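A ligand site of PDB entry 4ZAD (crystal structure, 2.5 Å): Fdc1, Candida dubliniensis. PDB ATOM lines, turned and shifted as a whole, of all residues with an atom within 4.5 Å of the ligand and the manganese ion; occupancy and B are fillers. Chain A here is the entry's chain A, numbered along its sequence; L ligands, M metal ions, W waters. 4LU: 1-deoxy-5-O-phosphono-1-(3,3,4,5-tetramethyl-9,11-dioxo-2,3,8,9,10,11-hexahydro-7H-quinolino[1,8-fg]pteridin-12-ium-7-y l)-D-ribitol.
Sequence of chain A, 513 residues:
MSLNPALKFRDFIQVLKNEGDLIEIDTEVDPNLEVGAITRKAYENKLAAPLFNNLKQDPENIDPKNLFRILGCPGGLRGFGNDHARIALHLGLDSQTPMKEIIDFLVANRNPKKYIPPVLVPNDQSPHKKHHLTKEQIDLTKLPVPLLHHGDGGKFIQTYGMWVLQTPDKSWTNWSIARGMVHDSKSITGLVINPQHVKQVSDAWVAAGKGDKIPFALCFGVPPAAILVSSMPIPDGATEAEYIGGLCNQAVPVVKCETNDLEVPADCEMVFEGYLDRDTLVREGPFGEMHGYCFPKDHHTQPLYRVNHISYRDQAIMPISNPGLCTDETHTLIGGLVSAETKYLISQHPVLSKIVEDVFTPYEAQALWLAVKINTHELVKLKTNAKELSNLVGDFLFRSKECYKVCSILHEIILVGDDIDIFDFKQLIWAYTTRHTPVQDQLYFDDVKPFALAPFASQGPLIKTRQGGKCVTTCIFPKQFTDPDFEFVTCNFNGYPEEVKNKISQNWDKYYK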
ATOM      1  N   GLN A 158      26.820  -2.878  20.083  1.00  0.00           N
ATOM      2  CA  GLN A 158      27.185  -1.463  19.976  1.00  0.00           C
ATOM      3  C   GLN A 158      26.150  -0.758  19.151  1.00  0.00           C
ATOM      4  O   GLN A 158      26.146  -0.800  17.918  1.00  0.00           O
ATOM      5  CB  GLN A 158      28.591  -1.317  19.413  1.00  0.00           C
ATOM      6  CG  GLN A 158      28.921  -0.050  18.657  1.00  0.00           C
ATOM      7  CD  GLN A 158      28.637   1.236  19.403  1.00  0.00           C
ATOM      8  OE1 GLN A 158      28.061   1.243  20.473  1.00  0.00           O
ATOM      9  NE2 GLN A 158      29.032   2.334  18.790  1.00  0.00           N
ATOM     10  N   THR A 159      25.241  -0.128  19.870  1.00  0.00           N
ATOM     11  CA  THR A 159      24.244   0.702  19.269  1.00  0.00           C
ATOM     12  C   THR A 159      24.216   2.079  19.912  1.00  0.00           C
ATOM     13  O   THR A 159      23.580   2.955  19.384  1.00  0.00           O
ATOM     14  CB  THR A 159      22.844   0.039  19.315  1.00  0.00           C
ATOM     15  OG1 THR A 159      22.345  -0.006  20.672  1.00  0.00           O
ATOM     16  CG2 THR A 159      22.912  -1.365  18.764  1.00  0.00           C
ATOM     17  N   TYR A 160      24.899   2.297  21.038  1.00  0.00           N
ATOM     18  CA  TYR A 160      24.822   3.610  21.691  1.00  0.00           C
ATOM     19  C   TYR A 160      26.008   3.880  22.586  1.00  0.00           C
ATOM     20  O   TYR A 160      25.912   4.569  23.627  1.00  0.00           O
ATOM     21  CB  TYR A 160      23.492   3.732  22.459  1.00  0.00           C
ATOM     22  CG  TYR A 160      22.962   5.164  22.622  1.00  0.00           C
ATOM     23  CD1 TYR A 160      22.255   5.774  21.618  1.00  0.00           C
ATOM     24  CD2 TYR A 160      23.148   5.880  23.814  1.00  0.00           C
ATOM     25  CE1 TYR A 160      21.748   7.084  21.780  1.00  0.00           C
ATOM     26  CE2 TYR A 160      22.644   7.162  23.983  1.00  0.00           C
ATOM     27  CZ  TYR A 160      21.947   7.758  22.963  1.00  0.00           C
ATOM     28  OH  TYR A 160      21.436   9.003  23.113  1.00  0.00           O
ATOM     29  N   ASN A 174      38.803  11.353  17.235  1.00  0.00           N
ATOM     30  CA  ASN A 174      37.410  11.352  16.834  1.00  0.00           C
ATOM     31  C   ASN A 174      36.551  10.500  17.758  1.00  0.00           C
ATOM     32  O   ASN A 174      36.946   9.402  18.124  1.00  0.00           O
ATOM     33  CB  ASN A 174      37.255  10.859  15.391  1.00  0.00           C
ATOM     34  CG  ASN A 174      35.918  11.229  14.792  1.00  0.00           C
ATOM     35  OD1 ASN A 174      35.740  12.327  14.251  1.00  0.00           O
ATOM     36  ND2 ASN A 174      34.944  10.307  14.897  1.00  0.00           N
ATOM     37  N   TRP A 175      35.385  11.022  18.138  1.00  0.00           N
ATOM     38  CA  TRP A 175      34.404  10.263  18.926  1.00  0.00           C
ATOM     39  C   TRP A 175      33.137  10.172  18.083  1.00  0.00           C
ATOM     40  O   TRP A 175      32.593  11.212  17.651  1.00  0.00           O
ATOM     41  CB  TRP A 175      34.081  10.975  20.246  1.00  0.00           C
ATOM     42  CG  TRP A 175      35.198  11.025  21.282  1.00  0.00           C
ATOM     43  CD1 TRP A 175      36.480  10.569  21.152  1.00  0.00           C
ATOM     44  CD2 TRP A 175      35.116  11.593  22.602  1.00  0.00           C
ATOM     45  NE1 TRP A 175      37.189  10.817  22.308  1.00  0.00           N
ATOM     46  CE2 TRP A 175      36.371  11.455  23.208  1.00  0.00           C
ATOM     47  CE3 TRP A 175      34.095  12.214  23.323  1.00  0.00           C
ATOM     48  CZ2 TRP A 175      36.640  11.892  24.504  1.00  0.00           C
ATOM     49  CZ3 TRP A 175      34.372  12.668  24.596  1.00  0.00           C
ATOM     50  CH2 TRP A 175      35.635  12.475  25.183  1.00  0.00           C
ATOM     51  N   SER A 176      32.682   8.960  17.800  1.00  0.00           N
ATOM     52  CA  SER A 176      31.484   8.788  16.984  1.00  0.00           C
ATOM     53  C   SER A 176      30.725   7.534  17.316  1.00  0.00           C
ATOM     54  O   SER A 176      31.227   6.676  18.023  1.00  0.00           O
ATOM     55  CB  SER A 176      31.868   8.740  15.529  1.00  0.00           C
ATOM     56  OG  SER A 176      32.642   7.602  15.300  1.00  0.00           O
ATOM     57  N   ILE A 177      29.505   7.415  16.786  1.00  0.00           N
ATOM     58  CA  ILE A 177      28.680   6.205  16.928  1.00  0.00           C
ATOM     59  C   ILE A 177      28.682   5.518  15.611  1.00  0.00           C
ATOM     60  O   ILE A 177      28.578   6.161  14.577  1.00  0.00           O
ATOM     61  CB  ILE A 177      27.204   6.498  17.273  1.00  0.00           C
ATOM     62  CG1 ILE A 177      27.067   7.245  18.589  1.00  0.00           C
ATOM     63  CG2 ILE A 177      26.362   5.198  17.298  1.00  0.00           C
ATOM     64  CD1 ILE A 177      25.620   7.618  18.911  1.00  0.00           C
ATOM     65  N   ALA A 178      28.789   4.200  15.656  1.00  0.00           N
ATOM     66  CA  ALA A 178      28.649   3.355  14.466  1.00  0.00           C
ATOM     67  C   ALA A 178      28.281   2.015  15.001  1.00  0.00           C
ATOM     68  O   ALA A 178      28.681   1.677  16.095  1.00  0.00           O
ATOM     69  CB  ALA A 178      29.961   3.281  13.646  1.00  0.00           C
ATOM     70  N   ARG A 179      27.517   1.264  14.238  1.00  0.00           N
ATOM     71  CA  ARG A 179      26.960   0.036  14.747  1.00  0.00           C
ATOM     72  C   ARG A 179      28.045  -0.984  14.882  1.00  0.00           C
ATOM     73  O   ARG A 179      29.123  -0.844  14.279  1.00  0.00           O
ATOM     74  CB  ARG A 179      25.847  -0.477  13.843  1.00  0.00           C
ATOM     75  CG  ARG A 179      26.295  -1.123  12.587  1.00  0.00           C
ATOM     76  CD  ARG A 179      25.061  -1.504  11.813  1.00  0.00           C
ATOM     77  NE  ARG A 179      25.314  -2.324  10.637  1.00  0.00           N
ATOM     78  CZ  ARG A 179      24.570  -2.284   9.536  1.00  0.00           C
ATOM     79  NH1 ARG A 179      23.533  -1.456   9.448  1.00  0.00           N
ATOM     80  NH2 ARG A 179      24.850  -3.069   8.502  1.00  0.00           N
ATOM     81  N   LEU A 191      29.952  -1.397  10.688  1.00  0.00           N
ATOM     82  CA  LEU A 191      30.161  -0.494   9.550  1.00  0.00           C
ATOM     83  C   LEU A 191      31.306   0.485   9.725  1.00  0.00           C
ATOM     84  O   LEU A 191      31.456   1.118  10.789  1.00  0.00           O
ATOM     85  CB  LEU A 191      28.901   0.334   9.315  1.00  0.00           C
ATOM     86  CG  LEU A 191      27.736  -0.241   8.522  1.00  0.00           C
ATOM     87  CD1 LEU A 191      26.663   0.833   8.530  1.00  0.00           C
ATOM     88  CD2 LEU A 191      28.161  -0.563   7.114  1.00  0.00           C
ATOM     89  N   GLN A 196      32.571   8.482   6.581  1.00  0.00           N
ATOM     90  CA  GLN A 196      32.499   8.555   8.031  1.00  0.00           C
ATOM     91  C   GLN A 196      33.866   8.663   8.683  1.00  0.00           C
ATOM     92  O   GLN A 196      34.844   8.068   8.231  1.00  0.00           O
ATOM     93  CB  GLN A 196      31.739   7.365   8.600  1.00  0.00           C
ATOM     94  CG  GLN A 196      30.313   7.298   8.104  1.00  0.00           C
ATOM     95  CD  GLN A 196      29.464   8.473   8.572  1.00  0.00           C
ATOM     96  OE1 GLN A 196      29.544   9.585   8.001  1.00  0.00           O
ATOM     97  NE2 GLN A 196      28.656   8.238   9.613  1.00  0.00           N
ATOM     98  N   HIS A 197      33.924   9.389   9.785  1.00  0.00           N
ATOM     99  CA  HIS A 197      35.204   9.569  10.425  1.00  0.00           C
ATOM    100  C   HIS A 197      35.897   8.298  10.918  1.00  0.00           C
ATOM    101  O   HIS A 197      37.118   8.223  10.859  1.00  0.00           O
ATOM    102  CB  HIS A 197      35.117  10.647  11.502  1.00  0.00           C
ATOM    103  CG  HIS A 197      34.925  12.024  10.926  1.00  0.00           C
ATOM    104  ND1 HIS A 197      35.165  12.281   9.603  1.00  0.00           N
ATOM    105  CD2 HIS A 197      34.580  13.192  11.492  1.00  0.00           C
ATOM    106  CE1 HIS A 197      34.955  13.557   9.366  1.00  0.00           C
ATOM    107  NE2 HIS A 197      34.590  14.141  10.495  1.00  0.00           N
ATOM    108  N   VAL A 198      35.151   7.286  11.360  1.00  0.00           N
ATOM    109  CA  VAL A 198      35.803   6.020  11.751  1.00  0.00           C
ATOM    110  C   VAL A 198      36.652   5.492  10.597  1.00  0.00           C
ATOM    111  O   VAL A 198      37.687   4.892  10.834  1.00  0.00           O
ATOM    112  CB  VAL A 198      34.827   4.912  12.219  1.00  0.00           C
ATOM    113  CG1 VAL A 198      34.249   5.239  13.570  1.00  0.00           C
ATOM    114  CG2 VAL A 198      33.731   4.733  11.240  1.00  0.00           C
ATOM    115  N   SER A 230      28.876  12.576  19.616  1.00  0.00           N
ATOM    116  CA  SER A 230      29.374  11.388  18.949  1.00  0.00           C
ATOM    117  C   SER A 230      28.470  11.103  17.747  1.00  0.00           C
ATOM    118  O   SER A 230      28.907  10.590  16.722  1.00  0.00           O
ATOM    119  CB  SER A 230      29.421  10.154  19.892  1.00  0.00           C
ATOM    120  OG  SER A 230      30.513  10.216  20.810  1.00  0.00           O
ATOM    121  N   SER A 231      27.230  11.488  17.865  1.00  0.00           N
ATOM    122  CA  SER A 231      26.297  11.318  16.774  1.00  0.00           C
ATOM    123  C   SER A 231      26.181  12.484  15.741  1.00  0.00           C
ATOM    124  O   SER A 231      25.488  12.356  14.742  1.00  0.00           O
ATOM    125  CB  SER A 231      24.946  10.992  17.386  1.00  0.00           C
ATOM    126  OG  SER A 231      24.026  10.728  16.330  1.00  0.00           O
ATOM    127  N   MET A 232      26.891  13.585  15.980  1.00  0.00           N
ATOM    128  CA  MET A 232      26.846  14.805  15.156  1.00  0.00           C
ATOM    129  C   MET A 232      28.027  14.884  14.196  1.00  0.00           C
ATOM    130  O   MET A 232      29.141  14.617  14.606  1.00  0.00           O
ATOM    131  CB  MET A 232      26.932  15.993  16.108  1.00  0.00           C
ATOM    132  CG  MET A 232      26.928  17.371  15.468  1.00  0.00           C
ATOM    133  SD  MET A 232      26.412  18.560  16.694  1.00  0.00           S
ATOM    134  CE  MET A 232      26.165  20.033  15.697  1.00  0.00           C
ATOM    135  N   PRO A 233      27.796  15.256  12.920  1.00  0.00           N
ATOM    136  CA  PRO A 233      28.906  15.373  11.974  1.00  0.00           C
ATOM    137  C   PRO A 233      29.578  16.736  12.021  1.00  0.00           C
ATOM    138  O   PRO A 233      29.370  17.576  11.126  1.00  0.00           O
ATOM    139  CB  PRO A 233      28.231  15.179  10.632  1.00  0.00           C
ATOM    140  CG  PRO A 233      26.889  15.779  10.830  1.00  0.00           C
ATOM    141  CD  PRO A 233      26.507  15.415  12.235  1.00  0.00           C
ATOM    142  N   ILE A 234      30.390  16.957  13.064  1.00  0.00           N
ATOM    143  CA  ILE A 234      31.256  18.145  13.128  1.00  0.00           C
ATOM    144  C   ILE A 234      32.439  17.962  12.149  1.00  0.00           C
ATOM    145  O   ILE A 234      32.594  16.906  11.511  1.00  0.00           O
ATOM    146  CB  ILE A 234      31.744  18.446  14.560  1.00  0.00           C
ATOM    147  CG1 ILE A 234      32.675  17.364  15.116  1.00  0.00           C
ATOM    148  CG2 ILE A 234      30.560  18.681  15.495  1.00  0.00           C
ATOM    149  CD1 ILE A 234      33.522  17.881  16.225  1.00  0.00           C
ATOM    150  N   ALA A 238      38.165  17.520  13.298  1.00  0.00           N
ATOM    151  CA  ALA A 238      37.758  18.147  14.545  1.00  0.00           C
ATOM    152  C   ALA A 238      37.687  17.150  15.713  1.00  0.00           C
ATOM    153  O   ALA A 238      37.066  16.090  15.580  1.00  0.00           O
ATOM    154  CB  ALA A 238      36.443  18.839  14.364  1.00  0.00           C
ATOM    155  N   GLU A 240      35.949  16.006  18.732  1.00  0.00           N
ATOM    156  CA  GLU A 240      34.648  16.137  19.388  1.00  0.00           C
ATOM    157  C   GLU A 240      34.772  16.569  20.850  1.00  0.00           C
ATOM    158  O   GLU A 240      34.010  17.430  21.306  1.00  0.00           O
ATOM    159  CB  GLU A 240      33.879  14.822  19.362  1.00  0.00           C
ATOM    160  CG  GLU A 240      33.211  14.483  18.062  1.00  0.00           C
ATOM    161  CD  GLU A 240      34.144  13.885  17.020  1.00  0.00           C
ATOM    162  OE1 GLU A 240      33.765  13.831  15.826  1.00  0.00           O
ATOM    163  OE2 GLU A 240      35.246  13.485  17.391  1.00  0.00           O
ATOM    164  N   PHE A 287      21.177  -5.317   9.626  1.00  0.00           N
ATOM    165  CA  PHE A 287      20.596  -4.772  10.845  1.00  0.00           C
ATOM    166  C   PHE A 287      19.330  -4.004  10.437  1.00  0.00           C
ATOM    167  O   PHE A 287      19.285  -3.382   9.380  1.00  0.00           O
ATOM    168  CB  PHE A 287      21.640  -3.845  11.468  1.00  0.00           C
ATOM    169  CG  PHE A 287      21.288  -3.316  12.806  1.00  0.00           C
ATOM    170  CD1 PHE A 287      20.982  -4.158  13.839  1.00  0.00           C
ATOM    171  CD2 PHE A 287      21.349  -1.959  13.056  1.00  0.00           C
ATOM    172  CE1 PHE A 287      20.696  -3.681  15.106  1.00  0.00           C
ATOM    173  CE2 PHE A 287      21.036  -1.440  14.291  1.00  0.00           C
ATOM    174  CZ  PHE A 287      20.706  -2.311  15.339  1.00  0.00           C
ATOM    175  N   GLU A 289      17.515  -0.906  10.438  1.00  0.00           N
ATOM    176  CA  GLU A 289      18.118   0.434  10.546  1.00  0.00           C
ATOM    177  C   GLU A 289      17.121   1.559  10.300  1.00  0.00           C
ATOM    178  O   GLU A 289      15.920   1.337  10.128  1.00  0.00           O
ATOM    179  CB  GLU A 289      19.348   0.561   9.602  1.00  0.00           C
ATOM    180  CG  GLU A 289      20.755   0.509  10.304  1.00  0.00           C
ATOM    181  CD  GLU A 289      21.352   1.872  10.699  1.00  0.00           C
ATOM    182  OE1 GLU A 289      20.602   2.832  10.996  1.00  0.00           O
ATOM    183  OE2 GLU A 289      22.602   1.953  10.729  1.00  0.00           O
ATOM    184  N   SER A 321      20.195   1.580  21.256  1.00  0.00           N
ATOM    185  CA  SER A 321      19.213   2.089  20.278  1.00  0.00           C
ATOM    186  C   SER A 321      18.771   1.013  19.272  1.00  0.00           C
ATOM    187  O   SER A 321      19.579   0.282  18.691  1.00  0.00           O
ATOM    188  CB  SER A 321      19.732   3.286  19.505  1.00  0.00           C
ATOM    189  OG  SER A 321      18.833   3.658  18.480  1.00  0.00           O
ATOM    190  N   PRO A 323      16.799   0.778  16.040  1.00  0.00           N
ATOM    191  CA  PRO A 323      16.292   1.620  14.993  1.00  0.00           C
ATOM    192  C   PRO A 323      15.191   0.966  14.189  1.00  0.00           C
ATOM    193  O   PRO A 323      15.204  -0.236  14.006  1.00  0.00           O
ATOM    194  CB  PRO A 323      17.520   1.839  14.088  1.00  0.00           C
ATOM    195  CG  PRO A 323      18.647   1.486  14.885  1.00  0.00           C
ATOM    196  CD  PRO A 323      18.169   0.356  15.711  1.00  0.00           C
ATOM    197  N   GLU A 329      16.310   7.275  18.130  1.00  0.00           N
ATOM    198  CA  GLU A 329      17.603   7.984  18.055  1.00  0.00           C
ATOM    199  C   GLU A 329      18.127   8.143  16.645  1.00  0.00           C
ATOM    200  O   GLU A 329      18.864   9.079  16.372  1.00  0.00           O
ATOM    201  CB  GLU A 329      18.727   7.277  18.835  1.00  0.00           C
ATOM    202  CG  GLU A 329      18.530   7.129  20.353  1.00  0.00           C
ATOM    203  CD  GLU A 329      17.475   6.105  20.719  1.00  0.00           C
ATOM    204  OE1 GLU A 329      17.293   5.093  19.993  1.00  0.00           O
ATOM    205  OE2 GLU A 329      16.823   6.337  21.766  1.00  0.00           O
ATOM    206  N   THR A 330      17.827   7.222  15.729  1.00  0.00           N
ATOM    207  CA  THR A 330      18.328   7.409  14.358  1.00  0.00           C
ATOM    208  C   THR A 330      17.504   8.476  13.654  1.00  0.00           C
ATOM    209  O   THR A 330      17.704   8.753  12.478  1.00  0.00           O
ATOM    210  CB  THR A 330      18.329   6.111  13.527  1.00  0.00           C
ATOM    211  OG1 THR A 330      16.995   5.552  13.463  1.00  0.00           O
ATOM    212  CG2 THR A 330      19.251   5.103  14.145  1.00  0.00           C
ATOM    213  N   LEU A 333      18.528  12.012  16.825  1.00  0.00           N
ATOM    214  CA  LEU A 333      19.940  12.322  16.895  1.00  0.00           C
ATOM    215  C   LEU A 333      20.575  12.339  15.499  1.00  0.00           C
ATOM    216  O   LEU A 333      21.364  13.233  15.203  1.00  0.00           O
ATOM    217  CB  LEU A 333      20.716  11.353  17.830  1.00  0.00           C
ATOM    218  CG  LEU A 333      20.493  11.417  19.341  1.00  0.00           C
ATOM    219  CD1 LEU A 333      21.446  10.480  20.030  1.00  0.00           C
ATOM    220  CD2 LEU A 333      20.672  12.868  19.872  1.00  0.00           C
ATOM    221  N   ILE A 334      20.275  11.381  14.646  1.00  0.00           N
ATOM    222  CA  ILE A 334      20.954  11.374  13.356  1.00  0.00           C
ATOM    223  C   ILE A 334      20.408  12.525  12.551  1.00  0.00           C
ATOM    224  O   ILE A 334      21.181  13.305  12.028  1.00  0.00           O
ATOM    225  CB  ILE A 334      20.838  10.041  12.597  1.00  0.00           C
ATOM    226  CG1 ILE A 334      21.603   8.932  13.324  1.00  0.00           C
ATOM    227  CG2 ILE A 334      21.356  10.221  11.145  1.00  0.00           C
ATOM    228  CD1 ILE A 334      21.564   7.597  12.616  1.00  0.00           C
ATOM    229  N   LYS A 405      29.927  15.486   3.415  1.00  0.00           N
ATOM    230  CA  LYS A 405      29.642  14.428   4.349  1.00  0.00           C
ATOM    231  C   LYS A 405      28.399  14.715   5.222  1.00  0.00           C
ATOM    232  O   LYS A 405      27.556  13.806   5.471  1.00  0.00           O
ATOM    233  CB  LYS A 405      30.838  14.256   5.283  1.00  0.00           C
ATOM    234  CG  LYS A 405      30.522  13.475   6.549  1.00  0.00           C
ATOM    235  CD  LYS A 405      31.770  13.066   7.326  1.00  0.00           C
ATOM    236  CE  LYS A 405      31.385  12.315   8.609  1.00  0.00           C
ATOM    237  NZ  LYS A 405      30.600  13.173   9.519  1.00  0.00           N
HETATM  238  C9  4LU L   1      23.902   7.274  14.828  1.00  0.00           C
HETATM  239  C8  4LU L   1      23.277   6.926  16.029  1.00  0.00           C
HETATM  240  C7  4LU L   1      22.995   5.583  16.335  1.00  0.00           C
HETATM  241  C10 4LU L   1      26.102   5.685  12.338  1.00  0.00           C
HETATM  242  C6  4LU L   1      23.293   4.559  15.287  1.00  0.00           C
HETATM  243  N3  4LU L   1      27.454   3.767  10.943  1.00  0.00           N
HETATM  244  C2  4LU L   1      27.834   5.040  10.836  1.00  0.00           C
HETATM  245  C13 4LU L   1      24.111   2.680  16.500  1.00  0.00           C
HETATM  246  C5  4LU L   1      23.035   3.132  15.530  1.00  0.00           C
HETATM  247  C1  4LU L   1      23.965   2.813  13.219  1.00  0.00           C
HETATM  248  O2  4LU L   1      28.802   5.298  10.110  1.00  0.00           O
HETATM  249  N1  4LU L   1      27.158   6.001  11.521  1.00  0.00           N
HETATM  250  C4  4LU L   1      26.406   3.400  11.716  1.00  0.00           C
HETATM  251  O4  4LU L   1      26.169   2.167  11.718  1.00  0.00           O
HETATM  252  C4A 4LU L   1      25.701   4.334  12.426  1.00  0.00           C
HETATM  253  N5  4LU L   1      24.274   4.068  13.057  1.00  0.00           N
HETATM  254  C3  4LU L   1      23.387   2.316  14.380  1.00  0.00           C
HETATM  255  C12 4LU L   1      21.666   2.822  16.129  1.00  0.00           C
HETATM  256  C5A 4LU L   1      23.905   5.001  14.006  1.00  0.00           C
HETATM  257  C7M 4LU L   1      22.356   5.150  17.623  1.00  0.00           C
HETATM  258  C8M 4LU L   1      22.996   8.047  17.000  1.00  0.00           C
HETATM  259  C9A 4LU L   1      24.366   6.332  13.895  1.00  0.00           C
HETATM  260  N10 4LU L   1      25.455   6.669  13.023  1.00  0.00           N
HETATM  261  C1' 4LU L   1      25.558   8.001  12.412  1.00  0.00           C
HETATM  262  C2' 4LU L   1      26.819   8.669  12.942  1.00  0.00           C
HETATM  263  O2' 4LU L   1      26.841   8.521  14.378  1.00  0.00           O
HETATM  264  C3' 4LU L   1      26.904  10.150  12.545  1.00  0.00           C
HETATM  265  O3' 4LU L   1      27.001  10.266  11.107  1.00  0.00           O
HETATM  266  C4' 4LU L   1      28.109  10.871  13.196  1.00  0.00           C
HETATM  267  O4' 4LU L   1      28.334  12.117  12.527  1.00  0.00           O
HETATM  268  C5' 4LU L   1      29.399  10.033  13.061  1.00  0.00           C
HETATM  269  O5' 4LU L   1      30.540  10.681  13.591  1.00  0.00           O
HETATM  270  P   4LU L   1      31.655  11.364  12.692  1.00  0.00           P
HETATM  271  O2P 4LU L   1      32.678  11.645  13.786  1.00  0.00           O
HETATM  272  O3P 4LU L   1      30.914  12.584  12.082  1.00  0.00           O
HETATM  273  O1P 4LU L   1      32.061  10.342  11.653  1.00  0.00           O
HETATM  274 MN    MN M   1      33.975  13.432  13.835  1.00  0.00          MN
HETATM  275  O   HOH W   1      28.254  11.844   9.058  1.00  0.00           O
HETATM  276  O   HOH W   2      32.251  14.661  12.951  1.00  0.00           O
HETATM  277  O   HOH W   3      31.057   3.675   9.369  1.00  0.00           O
HETATM  278  O   HOH W   4      35.300  15.359  13.770  1.00  0.00           O
HETATM  279  O   HOH W   5      32.451   8.025  12.592  1.00  0.00           O
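Water W2 lies within hydrogen-bond range of O3P of the ligand (2.6 Å), O of Ile 234 (2.7 Å) and NE2 of His 197 (3.4 Å).
Water W5 lies within hydrogen-bond range of an oxygen (O1P) of the ligand (2.5 Å), the side-chain hydroxyl of Ser 176 (2.7 Å), the backbone NH of Val 198 (3.1 Å) and the backbone NH of His 197 (3.5 Å).
Water W1 lies within hydrogen-bond range of NZ of Lys 405, OE1 of Gln 196 and O3' of the ligand.
Water W3 bridges O2 of the ligand (2.9 Å) and O of Leu 191 (3.0 Å).
The backbone NH (N) of His 197 is in hydrogen-bond range of an oxygen (O1P) of the ligand.
The side-chain amino group of Lys 405 lies within salt-bridge range of an oxygen (O3P) of the ligand (2.6 Å).
O2' of the ligand is in hydrogen-bond range of O of Ile 177, at 2.9 Å.
O2 of the ligand is in hydrogen-bond range of NE2 of Gln 196, at 3.0 Å.
An oxygen (O4) of the ligand is in hydrogen-bond range of the backbone NH of Arg 179 (3.0 Å).
The backbone carbonyl oxygen (O) of Met 232 sits close to an oxygen (O4') of the ligand (3.4 Å).
An oxygen (O4') of the ligand sits close to the backbone nitrogen (N) of Pro 233.
O of Thr 159 touches C13 of the ligand, at 2.9 Å.
O of Trp 175 touches O2P of the ligand, 3.9 Å away.
CB of Ser 176 touches O5' of the ligand, at 3.0 Å.
Ala 178 touches the ligand (CA to C4, 3.5 Å).
Leu 191 touches the ligand.
O of Ser 230 touches O5' of the ligand, 3.5 Å away.
Ser 231 touches the ligand (OG to C8M, 2.9 Å).
Glu 289 touches the ligand (OE2 to C1, 3.0 Å).
Ser 321 touches the ligand (CB to C7M, 3.7 Å).
Pro 323 touches the ligand (CG to C12, 3.5 Å).
CG2 of Thr 330 touches C12 of the ligand (3.9 Å).
CG1 of Ile 334 touches C9 of the ligand, at 3.2 Å.
Hydrophobic or aromatic side chains within 4 Å of the ligand: Ile 177, Ala 178, Leu 191, His 197, Pro 233, Pro 323 and Ile 334.
Merely in contact with the manganese ion: His 197 (2.4 Å).
Within 4 Å of the manganese ion: Asn 174, His 197 and Glu 240.
The nearest printed residue that does not touch the manganese ion is Ile 234 (4.3 Å).
The side-chain carboxylate (OE2) of Glu 240 lies within hydrogen-bond range of the backbone NH (N) of Trp 175.
The backbone NH (N) of Ile 177 lies within hydrogen-bond range of the backbone carbonyl oxygen (O) of Ser 230, at 3.2 Å.
N of Ser 321 lies within hydrogen-bond range of OG1 of Thr 159 (2.7 Å).
NH1 of Arg 179 lies within salt-bridge range of OE2 of Glu 289 (3.8 Å).
The backbone carbonyl oxygen of Glu 329 lies within hydrogen-bond range of the backbone NH of Ile 334 (3.2 Å).
The side-chain amide nitrogen (NE2) of Gln 158 sits at hydrogen-bond distance from the backbone carbonyl oxygen (O) of Ala 178.
OG of Ser 321 sits at hydrogen-bond distance from OE1 of Glu 329.
The manganese ion is bound by OE1 of Glu 240 (2.0 Å).
OD1 of Asn 174 binds the manganese ion (2.1 Å).
O2P of the ligand binds the manganese ion (2.2 Å).
Water W2 is bound to the manganese ion (2.3 Å).
Water W4 binds the manganese ion (2.3 Å).
The manganese ion has five donor atoms within binding distance.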
